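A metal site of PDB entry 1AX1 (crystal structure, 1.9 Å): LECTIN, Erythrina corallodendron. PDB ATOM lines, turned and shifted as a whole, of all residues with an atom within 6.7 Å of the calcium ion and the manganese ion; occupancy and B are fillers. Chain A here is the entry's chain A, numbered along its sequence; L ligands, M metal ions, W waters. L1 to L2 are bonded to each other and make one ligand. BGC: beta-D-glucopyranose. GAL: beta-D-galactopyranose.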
ATOM      1  N   ASP A  89     -12.956   7.846 -17.287  1.00  0.00           N
ATOM      2  CA  ASP A  89     -12.971   9.308 -17.268  1.00  0.00           C
ATOM      3  C   ASP A  89     -12.150   9.911 -18.401  1.00  0.00           C
ATOM      4  O   ASP A  89     -12.345  11.072 -18.788  1.00  0.00           O
ATOM      5  CB  ASP A  89     -12.431   9.842 -15.940  1.00  0.00           C
ATOM      6  CG  ASP A  89     -13.519  10.069 -14.917  1.00  0.00           C
ATOM      7  OD1 ASP A  89     -14.226  11.088 -15.020  1.00  0.00           O
ATOM      8  OD2 ASP A  89     -13.672   9.210 -14.026  1.00  0.00           O
ATOM      9  N   TYR A 106     -10.256   9.655 -11.258  1.00  0.00           N
ATOM     10  CA  TYR A 106     -11.541  10.103 -11.787  1.00  0.00           C
ATOM     11  C   TYR A 106     -11.378  11.283 -12.745  1.00  0.00           C
ATOM     12  O   TYR A 106     -10.499  11.256 -13.616  1.00  0.00           O
ATOM     13  CB  TYR A 106     -12.513  10.461 -10.648  1.00  0.00           C
ATOM     14  CG  TYR A 106     -12.557   9.427  -9.555  1.00  0.00           C
ATOM     15  CD1 TYR A 106     -12.685   8.075  -9.857  1.00  0.00           C
ATOM     16  CD2 TYR A 106     -12.437   9.797  -8.220  1.00  0.00           C
ATOM     17  CE1 TYR A 106     -12.668   7.109  -8.852  1.00  0.00           C
ATOM     18  CE2 TYR A 106     -12.411   8.852  -7.215  1.00  0.00           C
ATOM     19  CZ  TYR A 106     -12.530   7.514  -7.531  1.00  0.00           C
ATOM     20  OH  TYR A 106     -12.532   6.585  -6.521  1.00  0.00           O
ATOM     21  N   GLY A 107     -12.237  12.296 -12.596  1.00  0.00           N
ATOM     22  CA  GLY A 107     -12.208  13.471 -13.442  1.00  0.00           C
ATOM     23  C   GLY A 107     -10.907  14.239 -13.420  1.00  0.00           C
ATOM     24  O   GLY A 107     -10.668  15.084 -14.281  1.00  0.00           O
ATOM     25  N   TYR A 108     -10.051  13.965 -12.431  1.00  0.00           N
ATOM     26  CA  TYR A 108      -8.760  14.635 -12.311  1.00  0.00           C
ATOM     27  C   TYR A 108      -7.679  13.942 -13.122  1.00  0.00           C
ATOM     28  O   TYR A 108      -6.544  14.431 -13.209  1.00  0.00           O
ATOM     29  CB  TYR A 108      -8.379  14.799 -10.846  1.00  0.00           C
ATOM     30  CG  TYR A 108      -9.394  15.642 -10.105  1.00  0.00           C
ATOM     31  CD1 TYR A 108      -9.668  16.949 -10.520  1.00  0.00           C
ATOM     32  CD2 TYR A 108     -10.130  15.118  -9.045  1.00  0.00           C
ATOM     33  CE1 TYR A 108     -10.649  17.710  -9.894  1.00  0.00           C
ATOM     34  CE2 TYR A 108     -11.110  15.879  -8.419  1.00  0.00           C
ATOM     35  CZ  TYR A 108     -11.364  17.168  -8.855  1.00  0.00           C
ATOM     36  OH  TYR A 108     -12.337  17.916  -8.230  1.00  0.00           O
ATOM     37  N   LEU A 109      -8.052  12.806 -13.713  1.00  0.00           N
ATOM     38  CA  LEU A 109      -7.197  12.023 -14.592  1.00  0.00           C
ATOM     39  C   LEU A 109      -5.830  11.561 -14.056  1.00  0.00           C
ATOM     40  O   LEU A 109      -4.973  11.147 -14.831  1.00  0.00           O
ATOM     41  CB  LEU A 109      -7.016  12.772 -15.930  1.00  0.00           C
ATOM     42  CG  LEU A 109      -8.301  13.233 -16.636  1.00  0.00           C
ATOM     43  CD1 LEU A 109      -7.965  14.128 -17.813  1.00  0.00           C
ATOM     44  CD2 LEU A 109      -9.129  12.028 -17.087  1.00  0.00           C
ATOM     45  N   GLU A 127      -5.604  16.471 -22.787  1.00  0.00           N
ATOM     46  CA  GLU A 127      -6.547  15.430 -22.412  1.00  0.00           C
ATOM     47  C   GLU A 127      -7.492  14.965 -23.510  1.00  0.00           C
ATOM     48  O   GLU A 127      -7.732  15.654 -24.499  1.00  0.00           O
ATOM     49  CB  GLU A 127      -7.369  15.895 -21.220  1.00  0.00           C
ATOM     50  CG  GLU A 127      -8.210  17.133 -21.531  1.00  0.00           C
ATOM     51  CD  GLU A 127      -9.176  17.507 -20.429  1.00  0.00           C
ATOM     52  OE1 GLU A 127      -8.758  17.573 -19.267  1.00  0.00           O
ATOM     53  OE2 GLU A 127     -10.364  17.732 -20.744  1.00  0.00           O
ATOM     54  N   ASP A 129     -10.833  13.593 -22.793  1.00  0.00           N
ATOM     55  CA  ASP A 129     -11.861  13.521 -21.768  1.00  0.00           C
ATOM     56  C   ASP A 129     -13.177  12.891 -22.214  1.00  0.00           C
ATOM     57  O   ASP A 129     -13.865  13.436 -23.075  1.00  0.00           O
ATOM     58  CB  ASP A 129     -12.096  14.944 -21.264  1.00  0.00           C
ATOM     59  CG  ASP A 129     -12.760  14.990 -19.911  1.00  0.00           C
ATOM     60  OD1 ASP A 129     -13.354  13.992 -19.455  1.00  0.00           O
ATOM     61  OD2 ASP A 129     -12.688  16.064 -19.284  1.00  0.00           O
ATOM     62  N   THR A 130     -13.561  11.812 -21.551  1.00  0.00           N
ATOM     63  CA  THR A 130     -14.785  11.092 -21.899  1.00  0.00           C
ATOM     64  C   THR A 130     -15.994  11.306 -20.977  1.00  0.00           C
ATOM     65  O   THR A 130     -17.086  10.814 -21.282  1.00  0.00           O
ATOM     66  CB  THR A 130     -14.528   9.579 -22.016  1.00  0.00           C
ATOM     67  OG1 THR A 130     -14.048   9.069 -20.764  1.00  0.00           O
ATOM     68  CG2 THR A 130     -13.489   9.292 -23.103  1.00  0.00           C
ATOM     69  N   PHE A 131     -15.806  12.005 -19.863  1.00  0.00           N
ATOM     70  CA  PHE A 131     -16.911  12.259 -18.940  1.00  0.00           C
ATOM     71  C   PHE A 131     -17.022  13.741 -18.637  1.00  0.00           C
ATOM     72  O   PHE A 131     -16.038  14.388 -18.289  1.00  0.00           O
ATOM     73  CB  PHE A 131     -16.733  11.467 -17.638  1.00  0.00           C
ATOM     74  CG  PHE A 131     -17.862  11.670 -16.663  1.00  0.00           C
ATOM     75  CD1 PHE A 131     -17.837  12.716 -15.748  1.00  0.00           C
ATOM     76  CD2 PHE A 131     -18.978  10.832 -16.688  1.00  0.00           C
ATOM     77  CE1 PHE A 131     -18.886  12.941 -14.869  1.00  0.00           C
ATOM     78  CE2 PHE A 131     -20.035  11.036 -15.808  1.00  0.00           C
ATOM     79  CZ  PHE A 131     -19.990  12.103 -14.900  1.00  0.00           C
ATOM     80  N   SER A 132     -18.239  14.256 -18.727  1.00  0.00           N
ATOM     81  CA  SER A 132     -18.505  15.667 -18.479  1.00  0.00           C
ATOM     82  C   SER A 132     -18.707  16.030 -16.995  1.00  0.00           C
ATOM     83  O   SER A 132     -19.779  15.795 -16.431  1.00  0.00           O
ATOM     84  CB  SER A 132     -19.696  16.123 -19.329  1.00  0.00           C
ATOM     85  OG  SER A 132     -19.800  17.532 -19.343  1.00  0.00           O
ATOM     86  N   ASN A 133     -17.647  16.557 -16.373  1.00  0.00           N
ATOM     87  CA  ASN A 133     -17.675  16.992 -14.974  1.00  0.00           C
ATOM     88  C   ASN A 133     -18.237  18.416 -14.957  1.00  0.00           C
ATOM     89  O   ASN A 133     -18.438  19.020 -16.004  1.00  0.00           O
ATOM     90  CB  ASN A 133     -16.259  16.980 -14.388  1.00  0.00           C
ATOM     91  CG  ASN A 133     -15.654  15.589 -14.353  1.00  0.00           C
ATOM     92  OD1 ASN A 133     -14.943  15.185 -15.264  1.00  0.00           O
ATOM     93  ND2 ASN A 133     -15.919  14.859 -13.282  1.00  0.00           N
ATOM     94  N   TRP A 135     -16.875  21.157 -14.369  1.00  0.00           N
ATOM     95  CA  TRP A 135     -15.921  22.114 -14.939  1.00  0.00           C
ATOM     96  C   TRP A 135     -15.718  21.908 -16.448  1.00  0.00           C
ATOM     97  O   TRP A 135     -14.980  22.659 -17.087  1.00  0.00           O
ATOM     98  CB  TRP A 135     -14.570  22.002 -14.222  1.00  0.00           C
ATOM     99  CG  TRP A 135     -13.998  20.612 -14.268  1.00  0.00           C
ATOM    100  CD1 TRP A 135     -13.400  19.995 -15.345  1.00  0.00           C
ATOM    101  CD2 TRP A 135     -13.971  19.659 -13.198  1.00  0.00           C
ATOM    102  NE1 TRP A 135     -13.003  18.723 -15.003  1.00  0.00           N
ATOM    103  CE2 TRP A 135     -13.352  18.493 -13.693  1.00  0.00           C
ATOM    104  CE3 TRP A 135     -14.426  19.679 -11.881  1.00  0.00           C
ATOM    105  CZ2 TRP A 135     -13.156  17.342 -12.904  1.00  0.00           C
ATOM    106  CZ3 TRP A 135     -14.240  18.537 -11.082  1.00  0.00           C
ATOM    107  CH2 TRP A 135     -13.616  17.392 -11.602  1.00  0.00           C
ATOM    108  N   ASP A 136     -16.347  20.880 -17.006  1.00  0.00           N
ATOM    109  CA  ASP A 136     -16.219  20.549 -18.419  1.00  0.00           C
ATOM    110  C   ASP A 136     -17.320  21.098 -19.302  1.00  0.00           C
ATOM    111  O   ASP A 136     -18.396  21.477 -18.824  1.00  0.00           O
ATOM    112  CB  ASP A 136     -16.266  19.033 -18.606  1.00  0.00           C
ATOM    113  CG  ASP A 136     -14.970  18.361 -18.264  1.00  0.00           C
ATOM    114  OD1 ASP A 136     -13.911  18.928 -18.605  1.00  0.00           O
ATOM    115  OD2 ASP A 136     -15.011  17.259 -17.671  1.00  0.00           O
ATOM    116  N   PRO A 137     -17.050  21.205 -20.619  1.00  0.00           N
ATOM    117  CA  PRO A 137     -18.086  21.680 -21.523  1.00  0.00           C
ATOM    118  C   PRO A 137     -19.063  20.492 -21.576  1.00  0.00           C
ATOM    119  O   PRO A 137     -18.698  19.374 -21.183  1.00  0.00           O
ATOM    120  CB  PRO A 137     -17.328  21.867 -22.848  1.00  0.00           C
ATOM    121  CG  PRO A 137     -16.135  20.978 -22.714  1.00  0.00           C
ATOM    122  CD  PRO A 137     -15.738  21.187 -21.283  1.00  0.00           C
ATOM    123  N   VAL A 140     -18.876  15.558 -24.841  1.00  0.00           N
ATOM    124  CA  VAL A 140     -17.855  14.559 -24.565  1.00  0.00           C
ATOM    125  C   VAL A 140     -18.013  13.483 -25.637  1.00  0.00           C
ATOM    126  O   VAL A 140     -19.125  13.225 -26.098  1.00  0.00           O
ATOM    127  CB  VAL A 140     -17.967  13.921 -23.161  1.00  0.00           C
ATOM    128  CG1 VAL A 140     -17.455  14.875 -22.098  1.00  0.00           C
ATOM    129  CG2 VAL A 140     -19.404  13.512 -22.877  1.00  0.00           C
ATOM    130  N   HIS A 142     -13.963  15.055 -25.605  1.00  0.00           N
ATOM    131  CA  HIS A 142     -13.339  16.276 -26.096  1.00  0.00           C
ATOM    132  C   HIS A 142     -11.847  16.276 -25.805  1.00  0.00           C
ATOM    133  O   HIS A 142     -11.377  15.628 -24.866  1.00  0.00           O
ATOM    134  CB  HIS A 142     -13.997  17.543 -25.526  1.00  0.00           C
ATOM    135  CG  HIS A 142     -13.923  17.657 -24.024  1.00  0.00           C
ATOM    136  ND1 HIS A 142     -14.957  17.321 -23.184  1.00  0.00           N
ATOM    137  CD2 HIS A 142     -12.920  18.083 -23.222  1.00  0.00           C
ATOM    138  CE1 HIS A 142     -14.562  17.549 -21.918  1.00  0.00           C
ATOM    139  NE2 HIS A 142     -13.335  18.010 -21.897  1.00  0.00           N
ATOM    140  N   ILE A 143     -11.114  16.947 -26.690  1.00  0.00           N
ATOM    141  CA  ILE A 143      -9.679  17.109 -26.525  1.00  0.00           C
ATOM    142  C   ILE A 143      -9.583  18.407 -25.710  1.00  0.00           C
ATOM    143  O   ILE A 143     -10.397  19.322 -25.894  1.00  0.00           O
ATOM    144  CB  ILE A 143      -8.965  17.332 -27.879  1.00  0.00           C
ATOM    145  CG1 ILE A 143      -9.293  16.183 -28.841  1.00  0.00           C
ATOM    146  CG2 ILE A 143      -7.448  17.419 -27.672  1.00  0.00           C
ATOM    147  CD1 ILE A 143      -8.895  16.446 -30.278  1.00  0.00           C
ATOM    148  N   GLY A 144      -8.627  18.480 -24.798  1.00  0.00           N
ATOM    149  CA  GLY A 144      -8.482  19.680 -24.019  1.00  0.00           C
ATOM    150  C   GLY A 144      -7.034  20.002 -23.715  1.00  0.00           C
ATOM    151  O   GLY A 144      -6.219  19.100 -23.560  1.00  0.00           O
ATOM    152  N   ASP A 146      -4.766  21.541 -21.038  1.00  0.00           N
ATOM    153  CA  ASP A 146      -4.759  21.862 -19.606  1.00  0.00           C
ATOM    154  C   ASP A 146      -3.462  22.548 -19.173  1.00  0.00           C
ATOM    155  O   ASP A 146      -2.370  22.008 -19.380  1.00  0.00           O
ATOM    156  CB  ASP A 146      -4.943  20.590 -18.779  1.00  0.00           C
ATOM    157  CG  ASP A 146      -6.215  19.841 -19.111  1.00  0.00           C
ATOM    158  OD1 ASP A 146      -7.082  20.376 -19.822  1.00  0.00           O
ATOM    159  OD2 ASP A 146      -6.376  18.704 -18.648  1.00  0.00           O
ATOM    160  N   ILE A 150      -7.458  21.367 -14.434  1.00  0.00           N
ATOM    161  CA  ILE A 150      -8.250  20.374 -15.151  1.00  0.00           C
ATOM    162  C   ILE A 150      -9.294  21.114 -16.013  1.00  0.00           C
ATOM    163  O   ILE A 150      -9.891  20.541 -16.924  1.00  0.00           O
ATOM    164  CB  ILE A 150      -8.922  19.359 -14.165  1.00  0.00           C
ATOM    165  CG1 ILE A 150      -9.480  18.160 -14.934  1.00  0.00           C
ATOM    166  CG2 ILE A 150      -9.974  20.047 -13.310  1.00  0.00           C
ATOM    167  CD1 ILE A 150      -8.410  17.290 -15.595  1.00  0.00           C
ATOM    168  N   ARG A 151      -9.489  22.397 -15.722  1.00  0.00           N
ATOM    169  CA  ARG A 151     -10.410  23.241 -16.486  1.00  0.00           C
ATOM    170  C   ARG A 151      -9.610  23.743 -17.684  1.00  0.00           C
ATOM    171  O   ARG A 151      -8.897  24.734 -17.593  1.00  0.00           O
ATOM    172  CB  ARG A 151     -10.855  24.446 -15.654  1.00  0.00           C
ATOM    173  CG  ARG A 151     -11.541  24.115 -14.350  1.00  0.00           C
ATOM    174  CD  ARG A 151     -12.198  25.357 -13.776  1.00  0.00           C
ATOM    175  NE  ARG A 151     -11.552  25.830 -12.549  1.00  0.00           N
ATOM    176  CZ  ARG A 151     -10.878  26.968 -12.435  1.00  0.00           C
ATOM    177  NH1 ARG A 151     -10.725  27.772 -13.481  1.00  0.00           N
ATOM    178  NH2 ARG A 151     -10.338  27.293 -11.269  1.00  0.00           N
ATOM    179  N   SER A 152      -9.764  23.058 -18.825  1.00  0.00           N
ATOM    180  CA  SER A 152      -9.024  23.391 -20.039  1.00  0.00           C
ATOM    181  C   SER A 152      -9.135  24.839 -20.485  1.00  0.00           C
ATOM    182  O   SER A 152     -10.174  25.467 -20.304  1.00  0.00           O
ATOM    183  CB  SER A 152      -9.498  22.501 -21.190  1.00  0.00           C
ATOM    184  OG  SER A 152      -9.512  21.153 -20.794  1.00  0.00           O
ATOM    185  N   THR A 155     -10.927  23.780 -25.674  1.00  0.00           N
ATOM    186  CA  THR A 155     -11.549  22.466 -25.827  1.00  0.00           C
ATOM    187  C   THR A 155     -12.000  22.196 -27.267  1.00  0.00           C
ATOM    188  O   THR A 155     -12.339  23.127 -28.009  1.00  0.00           O
ATOM    189  CB  THR A 155     -12.733  22.327 -24.811  1.00  0.00           C
ATOM    190  OG1 THR A 155     -12.306  21.568 -23.678  1.00  0.00           O
ATOM    191  CG2 THR A 155     -13.944  21.701 -25.428  1.00  0.00           C
HETATM  192  C2  BGC L   1     -21.149   9.120  -7.601  1.00  0.00           C
HETATM  193  C3  BGC L   1     -19.861   9.289  -8.393  1.00  0.00           C
HETATM  194  C4  BGC L   1     -19.558  10.774  -8.609  1.00  0.00           C
HETATM  195  C5  BGC L   1     -19.578  11.502  -7.265  1.00  0.00           C
HETATM  196  C6  BGC L   1     -19.365  12.998  -7.379  1.00  0.00           C
HETATM  197  C1  BGC L   1     -21.068   9.926  -6.313  1.00  0.00           C
HETATM  198  O1  BGC L   1     -22.277   9.846  -5.640  1.00  0.00           O
HETATM  199  O2  BGC L   1     -21.356   7.744  -7.307  1.00  0.00           O
HETATM  200  O3  BGC L   1     -19.997   8.626  -9.643  1.00  0.00           O
HETATM  201  O4  BGC L   1     -18.245  10.932  -9.190  1.00  0.00           O
HETATM  202  O5  BGC L   1     -20.838  11.307  -6.607  1.00  0.00           O
HETATM  203  O6  BGC L   1     -20.047  13.530  -8.514  1.00  0.00           O
HETATM  204  C1  GAL L   2     -18.162  11.082 -10.570  1.00  0.00           C
HETATM  205  C2  GAL L   2     -16.762  11.615 -10.907  1.00  0.00           C
HETATM  206  C3  GAL L   2     -16.549  11.626 -12.428  1.00  0.00           C
HETATM  207  C4  GAL L   2     -16.799  10.211 -12.972  1.00  0.00           C
HETATM  208  C5  GAL L   2     -18.218   9.809 -12.587  1.00  0.00           C
HETATM  209  C6  GAL L   2     -18.588   8.429 -13.090  1.00  0.00           C
HETATM  210  O2  GAL L   2     -16.599  12.928 -10.388  1.00  0.00           O
HETATM  211  O3  GAL L   2     -15.222  12.025 -12.727  1.00  0.00           O
HETATM  212  O4  GAL L   2     -15.866   9.302 -12.419  1.00  0.00           O
HETATM  213  O5  GAL L   2     -18.356   9.784 -11.153  1.00  0.00           O
HETATM  214  O6  GAL L   2     -19.910   8.103 -12.707  1.00  0.00           O
HETATM  215 CA    CA M   1     -14.005  15.114 -17.421  1.00  0.00          CA
HETATM  216 MN    MN M   2     -12.306  18.126 -19.849  1.00  0.00          MN
HETATM  217  O   HOH W   1     -12.118  16.049 -16.382  1.00  0.00           O
HETATM  218  O   HOH W   2     -10.998  18.308 -17.833  1.00  0.00           O
HETATM  219  O   HOH W   3     -13.505  13.016 -16.808  1.00  0.00           O
HETATM  220  O   HOH W   4     -11.990  20.218 -20.295  1.00  0.00           O
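O3 of GAL L2 is in hydrogen-bond range of N of Gly 107 (3.0 Å).
The side-chain amide nitrogen of Asn 133 is in hydrogen-bond range of an oxygen (O3) of GAL L2, 3.0 Å away.
OD1 of Asp 89 lies within hydrogen-bond range of O3 of GAL L2, at 2.7 Å.
Water W1 lies within hydrogen-bond range of O of Gly 107 (2.7 Å) and NE1 of Trp 135 (3.1 Å).
Water W2 lies within hydrogen-bond range of the backbone carbonyl oxygen of Ile 150, the side-chain carboxylate of Glu 127 and the indole nitrogen of Trp 135.
The calcium ion is bound by water W3.
O of Phe 131 is bound to the calcium ion, 2.3 Å away.
The calcium ion is bound by water W1 (2.3 Å).
OD1 of Asn 133 is bound to the calcium ion (2.4 Å).
The calcium ion is bound by OD2 of Asp 136, at 2.4 Å.
The side-chain carboxylate (OD1) of Asp 129 is bound to the calcium ion, 2.4 Å away.
The side-chain carboxylate (OD2) of Asp 129 is bound to the calcium ion, 2.5 Å away.
The calcium ion has seven donor atoms within binding distance.
Four residues have an atom within 4 Å of the calcium ion: Asp 129, Phe 131, Asn 133 and Asp 136.
Along chain A the residues within 4 Å of the calcium ion span positions 129 to 136.
Four residues have an atom within 4 Å of the manganese ion: Glu 127, Asp 129, Asp 136 and His 142.
The nearest printed residue that does not touch the manganese ion is Ser 152 (4.2 Å).
OE1 of Glu 127 lies close to OD2 of Asp 146 (2.7 Å).
The backbone NH (N) of Glu 127 lies within hydrogen-bond range of the backbone carbonyl oxygen (O) of Gly 144 (2.8 Å).
The manganese ion is bound by water W4 (2.2 Å), OD2 of Asp 129 (2.2 Å), OE2 of Glu 127 (2.2 Å), OD1 of Asp 136 (2.2 Å), NE2 of His 142 (2.3 Å) and water W2 (2.4 Å).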
